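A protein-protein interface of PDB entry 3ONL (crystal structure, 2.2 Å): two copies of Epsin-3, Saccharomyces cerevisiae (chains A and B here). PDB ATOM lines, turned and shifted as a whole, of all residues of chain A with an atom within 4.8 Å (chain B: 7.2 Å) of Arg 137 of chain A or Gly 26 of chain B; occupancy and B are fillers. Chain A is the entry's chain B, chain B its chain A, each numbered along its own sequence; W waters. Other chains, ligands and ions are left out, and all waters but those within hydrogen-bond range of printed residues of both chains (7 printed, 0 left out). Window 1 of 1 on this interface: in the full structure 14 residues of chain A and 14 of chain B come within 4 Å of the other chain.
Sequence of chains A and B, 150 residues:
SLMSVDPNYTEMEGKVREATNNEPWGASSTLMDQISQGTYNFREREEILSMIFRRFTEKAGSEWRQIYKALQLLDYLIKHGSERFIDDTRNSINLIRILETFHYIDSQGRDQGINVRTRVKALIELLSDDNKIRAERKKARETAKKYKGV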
ATOM      1  N   LEU A  77       0.229  -8.939   8.257  1.00  0.00           N
ATOM      2  CA  LEU A  77       0.125  -9.624   6.966  1.00  0.00           C
ATOM      3  C   LEU A  77       1.313 -10.549   6.668  1.00  0.00           C
ATOM      4  O   LEU A  77       1.137 -11.620   6.074  1.00  0.00           O
ATOM      5  CB  LEU A  77      -0.112  -8.617   5.829  1.00  0.00           C
ATOM      6  CG  LEU A  77      -1.425  -7.819   5.913  1.00  0.00           C
ATOM      7  CD1 LEU A  77      -1.522  -6.771   4.814  1.00  0.00           C
ATOM      8  CD2 LEU A  77      -2.650  -8.752   5.886  1.00  0.00           C
ATOM      9  N   ILE A  78       2.508 -10.170   7.113  1.00  0.00           N
ATOM     10  CA  ILE A  78       3.687 -11.052   6.969  1.00  0.00           C
ATOM     11  C   ILE A  78       3.495 -12.332   7.781  1.00  0.00           C
ATOM     12  O   ILE A  78       3.925 -13.420   7.382  1.00  0.00           O
ATOM     13  CB  ILE A  78       4.987 -10.348   7.417  1.00  0.00           C
ATOM     14  CG1 ILE A  78       5.399  -9.304   6.385  1.00  0.00           C
ATOM     15  CG2 ILE A  78       6.149 -11.359   7.644  1.00  0.00           C
ATOM     16  CD1 ILE A  78       6.454  -8.388   6.890  1.00  0.00           C
ATOM     17  N   LYS A  79       2.835 -12.201   8.921  1.00  0.00           N
ATOM     18  CA  LYS A  79       2.652 -13.324   9.819  1.00  0.00           C
ATOM     19  C   LYS A  79       1.464 -14.218   9.469  1.00  0.00           C
ATOM     20  O   LYS A  79       1.492 -15.412   9.750  1.00  0.00           O
ATOM     21  CB  LYS A  79       2.557 -12.830  11.252  1.00  0.00           C
ATOM     22  CG  LYS A  79       3.895 -12.305  11.789  1.00  0.00           C
ATOM     23  CD  LYS A  79       3.700 -11.509  13.065  1.00  0.00           C
ATOM     24  CE  LYS A  79       5.022 -10.919  13.555  1.00  0.00           C
ATOM     25  NZ  LYS A  79       4.821 -10.000  14.715  1.00  0.00           N
ATOM     26  N   HIS A  80       0.439 -13.648   8.837  1.00  0.00           N
ATOM     27  CA  HIS A  80      -0.824 -14.357   8.630  1.00  0.00           C
ATOM     28  C   HIS A  80      -1.215 -14.539   7.171  1.00  0.00           C
ATOM     29  O   HIS A  80      -2.017 -15.415   6.844  1.00  0.00           O
ATOM     30  CB  HIS A  80      -1.957 -13.644   9.376  1.00  0.00           C
ATOM     31  CG  HIS A  80      -1.874 -13.791  10.861  1.00  0.00           C
ATOM     32  ND1 HIS A  80      -2.429 -14.857  11.533  1.00  0.00           N
ATOM     33  CD2 HIS A  80      -1.291 -13.011  11.803  1.00  0.00           C
ATOM     34  CE1 HIS A  80      -2.196 -14.728  12.827  1.00  0.00           C
ATOM     35  NE2 HIS A  80      -1.508 -13.614  13.018  1.00  0.00           N
ATOM     36  N   GLY A  81      -0.654 -13.711   6.300  1.00  0.00           N
ATOM     37  CA  GLY A  81      -1.075 -13.676   4.906  1.00  0.00           C
ATOM     38  C   GLY A  81      -0.293 -14.602   4.008  1.00  0.00           C
ATOM     39  O   GLY A  81       0.496 -15.423   4.474  1.00  0.00           O
ATOM     40  N   SER A  82      -0.497 -14.439   2.707  1.00  0.00           N
ATOM     41  CA  SER A  82       0.061 -15.336   1.704  1.00  0.00           C
ATOM     42  C   SER A  82       1.573 -15.190   1.560  1.00  0.00           C
ATOM     43  O   SER A  82       2.103 -14.088   1.666  1.00  0.00           O
ATOM     44  CB  SER A  82      -0.591 -15.030   0.347  1.00  0.00           C
ATOM     45  OG  SER A  82       0.083 -15.746  -0.669  1.00  0.00           O
ATOM     46  N   GLU A  83       2.261 -16.291   1.270  1.00  0.00           N
ATOM     47  CA  GLU A  83       3.707 -16.238   1.017  1.00  0.00           C
ATOM     48  C   GLU A  83       4.042 -15.355  -0.186  1.00  0.00           C
ATOM     49  O   GLU A  83       5.106 -14.739  -0.235  1.00  0.00           O
ATOM     50  CB  GLU A  83       4.287 -17.644   0.837  1.00  0.00           C
ATOM     51  CG  GLU A  83       4.245 -18.472   2.115  1.00  0.00           C
ATOM     52  CD  GLU A  83       5.060 -19.748   2.010  1.00  0.00           C
ATOM     53  OE1 GLU A  83       4.452 -20.839   1.997  1.00  0.00           O
ATOM     54  OE2 GLU A  83       6.307 -19.663   1.930  1.00  0.00           O
ATOM     55  N   ILE A  86       4.434 -11.883   1.033  1.00  0.00           N
ATOM     56  CA  ILE A  86       5.738 -11.703   1.673  1.00  0.00           C
ATOM     57  C   ILE A  86       6.785 -11.427   0.597  1.00  0.00           C
ATOM     58  O   ILE A  86       7.598 -10.516   0.720  1.00  0.00           O
ATOM     59  CB  ILE A  86       6.158 -12.944   2.507  1.00  0.00           C
ATOM     60  CG1 ILE A  86       5.205 -13.170   3.675  1.00  0.00           C
ATOM     61  CG2 ILE A  86       7.581 -12.783   3.077  1.00  0.00           C
ATOM     62  CD1 ILE A  86       5.366 -14.556   4.337  1.00  0.00           C
ATOM     63  N   ILE A 133      10.960 -15.148   9.792  1.00  0.00           N
ATOM     64  CA  ILE A 133       9.639 -15.224   9.154  1.00  0.00           C
ATOM     65  C   ILE A 133       8.975 -16.592   9.364  1.00  0.00           C
ATOM     66  O   ILE A 133       7.799 -16.677   9.754  1.00  0.00           O
ATOM     67  CB  ILE A 133       9.707 -14.910   7.647  1.00  0.00           C
ATOM     68  CG1 ILE A 133      10.161 -13.463   7.423  1.00  0.00           C
ATOM     69  CG2 ILE A 133       8.342 -15.139   7.004  1.00  0.00           C
ATOM     70  CD1 ILE A 133      10.614 -13.153   6.005  1.00  0.00           C
ATOM     71  N   ARG A 134       9.729 -17.659   9.107  1.00  0.00           N
ATOM     72  CA  ARG A 134       9.231 -19.021   9.336  1.00  0.00           C
ATOM     73  C   ARG A 134       8.782 -19.224  10.780  1.00  0.00           C
ATOM     74  O   ARG A 134       7.715 -19.785  11.031  1.00  0.00           O
ATOM     75  CB  ARG A 134      10.289 -20.060   8.961  1.00  0.00           C
ATOM     76  CG  ARG A 134      10.415 -20.285   7.473  1.00  0.00           C
ATOM     77  CD  ARG A 134      11.222 -21.544   7.157  1.00  0.00           C
ATOM     78  NE  ARG A 134      12.652 -21.334   7.335  1.00  0.00           N
ATOM     79  CZ  ARG A 134      13.472 -20.884   6.389  1.00  0.00           C
ATOM     80  NH1 ARG A 134      14.761 -20.729   6.655  1.00  0.00           N
ATOM     81  NH2 ARG A 134      13.014 -20.596   5.179  1.00  0.00           N
ATOM     82  N   ALA A 135       9.599 -18.747  11.717  1.00  0.00           N
ATOM     83  CA  ALA A 135       9.327 -18.878  13.145  1.00  0.00           C
ATOM     84  C   ALA A 135       8.127 -18.048  13.589  1.00  0.00           C
ATOM     85  O   ALA A 135       7.342 -18.500  14.426  1.00  0.00           O
ATOM     86  CB  ALA A 135      10.561 -18.521  13.961  1.00  0.00           C
ATOM     87  N   GLU A 136       7.965 -16.849  13.025  1.00  0.00           N
ATOM     88  CA  GLU A 136       6.784 -16.049  13.346  1.00  0.00           C
ATOM     89  C   GLU A 136       5.501 -16.644  12.762  1.00  0.00           C
ATOM     90  O   GLU A 136       4.439 -16.545  13.371  1.00  0.00           O
ATOM     91  CB  GLU A 136       6.954 -14.580  12.923  1.00  0.00           C
ATOM     92  CG  GLU A 136       8.050 -13.820  13.694  1.00  0.00           C
ATOM     93  CD  GLU A 136       7.643 -13.394  15.102  1.00  0.00           C
ATOM     94  OE1 GLU A 136       6.503 -13.674  15.527  1.00  0.00           O
ATOM     95  OE2 GLU A 136       8.473 -12.763  15.788  1.00  0.00           O
ATOM     96  N   ARG A 137       5.600 -17.266  11.590  1.00  0.00           N
ATOM     97  CA  ARG A 137       4.429 -17.842  10.947  1.00  0.00           C
ATOM     98  C   ARG A 137       3.951 -19.071  11.708  1.00  0.00           C
ATOM     99  O   ARG A 137       2.755 -19.287  11.850  1.00  0.00           O
ATOM    100  CB  ARG A 137       4.716 -18.215   9.493  1.00  0.00           C
ATOM    101  CG  ARG A 137       5.294 -17.101   8.644  1.00  0.00           C
ATOM    102  CD  ARG A 137       4.993 -17.312   7.185  1.00  0.00           C
ATOM    103  NE  ARG A 137       4.082 -16.265   6.831  1.00  0.00           N
ATOM    104  CZ  ARG A 137       3.009 -16.379   6.072  1.00  0.00           C
ATOM    105  NH1 ARG A 137       2.651 -17.531   5.504  1.00  0.00           N
ATOM    106  NH2 ARG A 137       2.301 -15.286   5.893  1.00  0.00           N
ATOM    107  N   LYS A 138       4.894 -19.874  12.184  1.00  0.00           N
ATOM    108  CA  LYS A 138       4.582 -21.055  12.987  1.00  0.00           C
ATOM    109  C   LYS A 138       3.989 -20.662  14.340  1.00  0.00           C
ATOM    110  O   LYS A 138       2.997 -21.236  14.784  1.00  0.00           O
ATOM    111  CB  LYS A 138       5.839 -21.906  13.198  1.00  0.00           C
ATOM    112  CG  LYS A 138       6.262 -22.701  11.977  1.00  0.00           C
ATOM    113  N   LYS A 139       4.608 -19.670  14.973  1.00  0.00           N
ATOM    114  CA  LYS A 139       4.212 -19.166  16.289  1.00  0.00           C
ATOM    115  C   LYS A 139       2.802 -18.570  16.268  1.00  0.00           C
ATOM    116  O   LYS A 139       2.081 -18.622  17.266  1.00  0.00           O
ATOM    117  CB  LYS A 139       5.240 -18.127  16.763  1.00  0.00           C
ATOM    118  CG  LYS A 139       4.921 -17.409  18.065  1.00  0.00           C
ATOM    119  CD  LYS A 139       5.966 -16.326  18.329  1.00  0.00           C
ATOM    120  N   ALA A 140       2.415 -18.003  15.127  1.00  0.00           N
ATOM    121  CA  ALA A 140       1.063 -17.487  14.953  1.00  0.00           C
ATOM    122  C   ALA A 140       0.056 -18.642  15.008  1.00  0.00           C
ATOM    123  O   ALA A 140      -1.058 -18.475  15.523  1.00  0.00           O
ATOM    124  CB  ALA A 140       0.947 -16.709  13.645  1.00  0.00           C
ATOM    125  N   ARG A 141       0.477 -19.807  14.503  1.00  0.00           N
ATOM    126  CA  ARG A 141      -0.311 -21.047  14.532  1.00  0.00           C
ATOM    127  C   ARG A 141      -0.341 -21.688  15.916  1.00  0.00           C
ATOM    128  O   ARG A 141      -1.377 -22.218  16.333  1.00  0.00           O
ATOM    129  CB  ARG A 141       0.221 -22.059  13.507  1.00  0.00           C
ATOM    130  N   GLU B  18      -1.319 -23.813  -2.841  1.00  0.00           N
ATOM    131  CA  GLU B  18      -0.762 -22.660  -2.130  1.00  0.00           C
ATOM    132  C   GLU B  18       0.003 -23.095  -0.877  1.00  0.00           C
ATOM    133  O   GLU B  18       1.142 -22.678  -0.659  1.00  0.00           O
ATOM    134  CB  GLU B  18      -1.885 -21.686  -1.768  1.00  0.00           C
ATOM    135  CG  GLU B  18      -1.473 -20.525  -0.865  1.00  0.00           C
ATOM    136  CD  GLU B  18      -1.054 -19.287  -1.632  1.00  0.00           C
ATOM    137  OE1 GLU B  18      -1.610 -19.036  -2.718  1.00  0.00           O
ATOM    138  OE2 GLU B  18      -0.180 -18.550  -1.132  1.00  0.00           O
ATOM    139  N   ALA B  19      -0.610 -23.960  -0.074  1.00  0.00           N
ATOM    140  CA  ALA B  19       0.008 -24.396   1.177  1.00  0.00           C
ATOM    141  C   ALA B  19       1.261 -25.219   0.933  1.00  0.00           C
ATOM    142  O   ALA B  19       2.030 -25.447   1.854  1.00  0.00           O
ATOM    143  CB  ALA B  19      -0.980 -25.168   2.036  1.00  0.00           C
ATOM    144  N   ASN B  21       3.382 -24.634  -2.047  1.00  0.00           N
ATOM    145  CA  ASN B  21       4.193 -23.986  -3.088  1.00  0.00           C
ATOM    146  C   ASN B  21       5.688 -23.929  -2.723  1.00  0.00           C
ATOM    147  O   ASN B  21       6.073 -24.312  -1.614  1.00  0.00           O
ATOM    148  CB  ASN B  21       3.629 -22.594  -3.455  1.00  0.00           C
ATOM    149  CG  ASN B  21       3.852 -21.539  -2.368  1.00  0.00           C
ATOM    150  OD1 ASN B  21       4.679 -21.698  -1.468  1.00  0.00           O
ATOM    151  ND2 ASN B  21       3.103 -20.440  -2.461  1.00  0.00           N
ATOM    152  N   GLU B  23       7.713 -21.427  -2.070  1.00  0.00           N
ATOM    153  CA  GLU B  23       8.207 -20.317  -1.240  1.00  0.00           C
ATOM    154  C   GLU B  23       8.781 -20.844   0.092  1.00  0.00           C
ATOM    155  O   GLU B  23       8.365 -21.897   0.573  1.00  0.00           O
ATOM    156  CB  GLU B  23       7.123 -19.248  -1.016  1.00  0.00           C
ATOM    157  CG  GLU B  23       6.431 -18.741  -2.297  1.00  0.00           C
ATOM    158  CD  GLU B  23       7.153 -17.581  -2.996  1.00  0.00           C
ATOM    159  OE1 GLU B  23       6.484 -16.854  -3.765  1.00  0.00           O
ATOM    160  OE2 GLU B  23       8.371 -17.385  -2.793  1.00  0.00           O
ATOM    161  N   PRO B  24       9.760 -20.126   0.673  1.00  0.00           N
ATOM    162  CA  PRO B  24      10.473 -20.658   1.836  1.00  0.00           C
ATOM    163  C   PRO B  24       9.902 -20.346   3.217  1.00  0.00           C
ATOM    164  O   PRO B  24      10.520 -20.705   4.214  1.00  0.00           O
ATOM    165  CB  PRO B  24      11.852 -20.017   1.701  1.00  0.00           C
ATOM    166  CG  PRO B  24      11.563 -18.703   1.086  1.00  0.00           C
ATOM    167  CD  PRO B  24      10.445 -18.945   0.113  1.00  0.00           C
ATOM    168  N   TRP B  25       8.735 -19.716   3.292  1.00  0.00           N
ATOM    169  CA  TRP B  25       8.259 -19.187   4.576  1.00  0.00           C
ATOM    170  C   TRP B  25       7.193 -20.005   5.294  1.00  0.00           C
ATOM    171  O   TRP B  25       6.945 -19.778   6.478  1.00  0.00           O
ATOM    172  CB  TRP B  25       7.828 -17.731   4.426  1.00  0.00           C
ATOM    173  CG  TRP B  25       8.897 -16.911   3.788  1.00  0.00           C
ATOM    174  CD1 TRP B  25      10.149 -16.639   4.292  1.00  0.00           C
ATOM    175  CD2 TRP B  25       8.831 -16.274   2.513  1.00  0.00           C
ATOM    176  NE1 TRP B  25      10.852 -15.855   3.409  1.00  0.00           N
ATOM    177  CE2 TRP B  25      10.071 -15.624   2.304  1.00  0.00           C
ATOM    178  CE3 TRP B  25       7.842 -16.184   1.522  1.00  0.00           C
ATOM    179  CZ2 TRP B  25      10.342 -14.885   1.151  1.00  0.00           C
ATOM    180  CZ3 TRP B  25       8.112 -15.454   0.376  1.00  0.00           C
ATOM    181  CH2 TRP B  25       9.352 -14.811   0.200  1.00  0.00           C
ATOM    182  N   GLY B  26       6.575 -20.947   4.585  1.00  0.00           N
ATOM    183  CA  GLY B  26       5.564 -21.826   5.177  1.00  0.00           C
ATOM    184  C   GLY B  26       4.143 -21.311   5.063  1.00  0.00           C
ATOM    185  O   GLY B  26       3.910 -20.104   5.048  1.00  0.00           O
ATOM    186  N   ALA B  27       3.189 -22.237   4.983  1.00  0.00           N
ATOM    187  CA  ALA B  27       1.760 -21.890   4.941  1.00  0.00           C
ATOM    188  C   ALA B  27       1.335 -21.227   6.233  1.00  0.00           C
ATOM    189  O   ALA B  27       1.805 -21.607   7.303  1.00  0.00           O
ATOM    190  CB  ALA B  27       0.911 -23.134   4.685  1.00  0.00           C
ATOM    191  N   SER B  28       0.451 -20.235   6.140  1.00  0.00           N
ATOM    192  CA  SER B  28      -0.035 -19.553   7.337  1.00  0.00           C
ATOM    193  C   SER B  28      -0.935 -20.459   8.169  1.00  0.00           C
ATOM    194  O   SER B  28      -1.495 -21.433   7.667  1.00  0.00           O
ATOM    195  CB  SER B  28      -0.800 -18.275   6.986  1.00  0.00           C
ATOM    196  OG  SER B  28      -2.125 -18.577   6.589  1.00  0.00           O
ATOM    197  N   SER B  29      -1.060 -20.105   9.442  1.00  0.00           N
ATOM    198  CA  SER B  29      -1.956 -20.756  10.393  1.00  0.00           C
ATOM    199  C   SER B  29      -3.396 -20.841   9.905  1.00  0.00           C
ATOM    200  O   SER B  29      -4.044 -21.888  10.021  1.00  0.00           O
ATOM    201  CB  SER B  29      -1.912 -19.978  11.715  1.00  0.00           C
ATOM    202  OG  SER B  29      -3.035 -20.265  12.527  1.00  0.00           O
ATOM    203  N   THR B  30      -3.897 -19.727   9.372  1.00  0.00           N
ATOM    204  CA  THR B  30      -5.276 -19.634   8.929  1.00  0.00           C
ATOM    205  C   THR B  30      -5.550 -20.445   7.664  1.00  0.00           C
ATOM    206  O   THR B  30      -6.637 -21.011   7.530  1.00  0.00           O
ATOM    207  CB  THR B  30      -5.713 -18.162   8.723  1.00  0.00           C
ATOM    208  OG1 THR B  30      -5.855 -17.531  10.000  1.00  0.00           O
ATOM    209  CG2 THR B  30      -7.040 -18.090   7.998  1.00  0.00           C
ATOM    210  N   LEU B  31      -4.581 -20.504   6.750  1.00  0.00           N
ATOM    211  CA  LEU B  31      -4.709 -21.341   5.547  1.00  0.00           C
ATOM    212  C   LEU B  31      -4.819 -22.813   5.934  1.00  0.00           C
ATOM    213  O   LEU B  31      -5.738 -23.523   5.504  1.00  0.00           O
ATOM    214  CB  LEU B  31      -3.521 -21.150   4.597  1.00  0.00           C
ATOM    215  CG  LEU B  31      -3.595 -21.955   3.291  1.00  0.00           C
ATOM    216  CD1 LEU B  31      -4.849 -21.596   2.478  1.00  0.00           C
ATOM    217  CD2 LEU B  31      -2.336 -21.732   2.459  1.00  0.00           C
ATOM    218  N   MET B  32      -3.874 -23.268   6.747  1.00  0.00           N
ATOM    219  CA  MET B  32      -3.919 -24.634   7.282  1.00  0.00           C
ATOM    220  C   MET B  32      -5.241 -24.962   7.985  1.00  0.00           C
ATOM    221  O   MET B  32      -5.822 -26.020   7.758  1.00  0.00           O
ATOM    222  CB  MET B  32      -2.744 -24.873   8.220  1.00  0.00           C
ATOM    223  CG  MET B  32      -1.414 -24.832   7.507  1.00  0.00           C
ATOM    224  SD  MET B  32      -0.159 -25.829   8.340  1.00  0.00           S
ATOM    225  CE  MET B  32       1.348 -25.170   7.641  1.00  0.00           C
ATOM    226  N   ARG B  65      11.256 -28.427  -0.849  1.00  0.00           N
ATOM    227  CA  ARG B  65      10.506 -27.670   0.141  1.00  0.00           C
ATOM    228  C   ARG B  65       9.010 -27.865  -0.043  1.00  0.00           C
ATOM    229  O   ARG B  65       8.254 -27.747   0.912  1.00  0.00           O
ATOM    230  CB  ARG B  65      10.887 -26.182   0.154  1.00  0.00           C
ATOM    231  CG  ARG B  65      10.449 -25.490   1.448  1.00  0.00           C
ATOM    232  CD  ARG B  65      10.849 -24.036   1.506  1.00  0.00           C
ATOM    233  NE  ARG B  65      12.253 -23.838   1.871  1.00  0.00           N
ATOM    234  CZ  ARG B  65      12.742 -23.951   3.105  1.00  0.00           C
ATOM    235  NH1 ARG B  65      11.956 -24.286   4.122  1.00  0.00           N
ATOM    236  NH2 ARG B  65      14.027 -23.731   3.322  1.00  0.00           N
ATOM    237  N   LYS B  69       6.698 -29.042   2.875  1.00  0.00           N
ATOM    238  CA  LYS B  69       5.473 -28.336   3.224  1.00  0.00           C
ATOM    239  C   LYS B  69       4.243 -29.247   3.182  1.00  0.00           C
ATOM    240  O   LYS B  69       3.344 -29.114   4.012  1.00  0.00           O
ATOM    241  CB  LYS B  69       5.306 -27.091   2.354  1.00  0.00           C
ATOM    242  CG  LYS B  69       6.246 -25.975   2.791  1.00  0.00           C
ATOM    243  CD  LYS B  69       6.522 -24.970   1.680  1.00  0.00           C
ATOM    244  CE  LYS B  69       5.442 -23.933   1.582  1.00  0.00           C
ATOM    245  NZ  LYS B  69       5.821 -22.861   0.627  1.00  0.00           N
ATOM    246  N   GLN B  72       4.266 -31.031   6.385  1.00  0.00           N
ATOM    247  CA  GLN B  72       3.788 -30.121   7.426  1.00  0.00           C
ATOM    248  C   GLN B  72       2.267 -30.048   7.437  1.00  0.00           C
ATOM    249  O   GLN B  72       1.639 -30.145   8.495  1.00  0.00           O
ATOM    250  CB  GLN B  72       4.337 -28.714   7.206  1.00  0.00           C
ATOM    251  CG  GLN B  72       5.774 -28.511   7.616  1.00  0.00           C
ATOM    252  CD  GLN B  72       6.197 -27.066   7.455  1.00  0.00           C
ATOM    253  OE1 GLN B  72       6.269 -26.554   6.337  1.00  0.00           O
ATOM    254  NE2 GLN B  72       6.473 -26.398   8.576  1.00  0.00           N
HETATM  255  O   HOH W   1      -5.306 -14.830  10.257  1.00  0.00           O
HETATM  256  O   HOH W   2       0.812 -18.025  10.220  1.00  0.00           O
HETATM  257  O   HOH W   3       0.972 -18.687   1.252  1.00  0.00           O
HETATM  258  O   HOH W   4       1.841 -21.203   1.636  1.00  0.00           O
HETATM  259  O   HOH W   5       6.457 -21.058   8.693  1.00  0.00           O
HETATM  260  O   HOH W   6      -2.616 -17.008   9.842  1.00  0.00           O
HETATM  261  O   HOH W   7      -4.046 -17.045   5.764  1.00  0.00           O
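N of Gly 26 of chain B lies within hydrogen-bond range of OE2 of Glu 83 of chain A, at 3.0 Å.
The side-chain carboxylate (OE1) of Glu 83 of chain A lies within salt-bridge range of the side-chain amino group (NZ) of Lys 69 of chain B, 2.8 Å away.
The side-chain carboxylate of Glu 18 of chain B is in hydrogen-bond range of the side-chain hydroxyl of Ser 82 of chain A, at 2.9 Å.
The backbone carbonyl oxygen (O) of His 80 of chain A sits close to the side-chain hydroxyl (OG) of Ser 28 of chain B, at 3.2 Å.
N of Trp 25 of chain B sits at hydrogen-bond distance from OE2 of Glu 83 of chain A (2.8 Å).
OE2 of Glu 83 of chain A sits close to O of Glu 23 of chain B, at 3.3 Å.
The guanidinium group (NH1) of Arg 137 of chain A lies within hydrogen-bond range of the backbone carbonyl oxygen (O) of Gly 26 of chain B (2.9 Å).
The backbone carbonyl oxygen (O) of Pro 24 of chain B is in hydrogen-bond range of the guanidinium group (NH2) of Arg 134 of chain A (2.7 Å).
No position is printed for both chains.
Of the printed residues of chain B, Arg 137 of chain A touches Trp 25, Gly 26, Ala 27 and Ser 28.
Printed residues of chain A within 4 Å of Gly 26 of chain B: Glu 83 and Arg 137.
Printed residues of chain A within 4 Å of Ser 28 of chain B: His 80 (3.1 Å) and Arg 137 (3.5 Å).
Of the printed residues of chain A, Glu 18 of chain B touches Ser 82.
Printed residues of chain A within 4 Å of Trp 25 of chain B: Glu 83 (2.8 Å), Ile 86 (3.7 Å), Ile 133 (3.6 Å), Arg 134 (3.6 Å) and Arg 137 (3.2 Å).
The nearest printed residue of chain B that does not touch Arg 137 of chain A is Ser 29 of chain B (4.6 Å).
The nearest printed residue of chain A that does not touch Gly 26 of chain B is Arg 134 of chain A (4.9 Å).
The nearest printed residue of chain A that does not touch Glu 23 of chain B is Arg 134 of chain A (6.6 Å).
O of Ile 78 of chain A lies within hydrogen-bond range of NH2 of Arg 137 of chain A (2.9 Å).
The side-chain amide nitrogen (ND2) of Asn 21 of chain B sits close to the backbone carbonyl oxygen (O) of Glu 18 of chain B (3.5 Å).
NZ of Lys 69 of chain B is in hydrogen-bond range of O of Glu 23 of chain B (2.7 Å).
N of Glu 23 of chain B sits at hydrogen-bond distance from OD1 of Asn 21 of chain B (3.1 Å).
The side-chain amide oxygen (OD1) of Asn 21 of chain B is in hydrogen-bond range of the side-chain amino group (NZ) of Lys 69 of chain B.
OG of Ser 28 of chain B sits at hydrogen-bond distance from N of Leu 31 of chain B, at 3.1 Å.
Among the printed residues, merely in contact across the chains: Glu 83 of chain A with Asn 21 of chain B (3.6 Å), Glu 83 of chain A with Pro 24 of chain B (3.7 Å), Glu 83 of chain A with Ala 27 of chain B (3.5 Å), Ile 86 of chain A with Trp 25 of chain B (3.7 Å), Ile 133 of chain A with Trp 25 of chain B (3.6 Å), Arg 134 of chain A with Trp 25 of chain B (3.6 Å), Arg 134 of chain A with Arg 65 of chain B (3.8 Å), Arg 137 of chain A with Trp 25 of chain B (3.2 Å), Arg 137 of chain A with Ala 27 of chain B (3.99 Å), Arg 137 of chain A with Ser 28 of chain B (3.5 Å) and Arg 141 of chain A with Ser 29 of chain B (3.4 Å).
Printed residues of chain A that touch a printed residue of chain B: His 80, Ser 82, Glu 83, Ile 86, Ile 133, Arg 134, Arg 137 and Arg 141.
Hydrophobic or aromatic side chains of chain A that line the printed part of chain B: Ile 86 and Ile 133.
Of the 16 printed residues of chain B, 11 touch a printed residue of chain A.
Hydrophobic or aromatic side chains of chain B within 4 Å of the printed part of chain A: Pro 24 and Trp 25.
Among the printed residues, 19 pairs touch across the chains.
Among the printed residues, Asp or Glu carboxylates within 4 Å of a Lys or Arg side-chain nitrogen of the other chain: Glu 83 of chain A with Lys 69 of chain B.
Water W7 bridges OG of Ser 28 of chain B (2.6 Å) and O of His 80 of chain A (2.8 Å).
Water W3 bridges OE2 of Glu 18 of chain B (2.7 Å) and N of Glu 83 of chain A (2.7 Å).
Water W4 lies within hydrogen-bond range of the side-chain carboxylate of Glu 83 of chain A (2.7 Å) and the backbone carbonyl oxygen of Glu 18 of chain B (2.8 Å).
Water W2 lies within hydrogen-bond range of the backbone carbonyl oxygen (O) of Lys 79 of chain A, the backbone carbonyl oxygen (O) of Arg 137 of chain A and the backbone NH (N) of Ser 29 of chain B.
Water W6 lies within hydrogen-bond range of a ring nitrogen (ND1) of His 80 of chain A (2.7 Å), the backbone NH of Thr 30 of chain B (3.0 Å) and the backbone NH of Ser 29 of chain B (3.5 Å).
Water W1 bridges OG1 of Thr 30 of chain B (2.8 Å) and ND1 of His 80 of chain A (3.1 Å).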
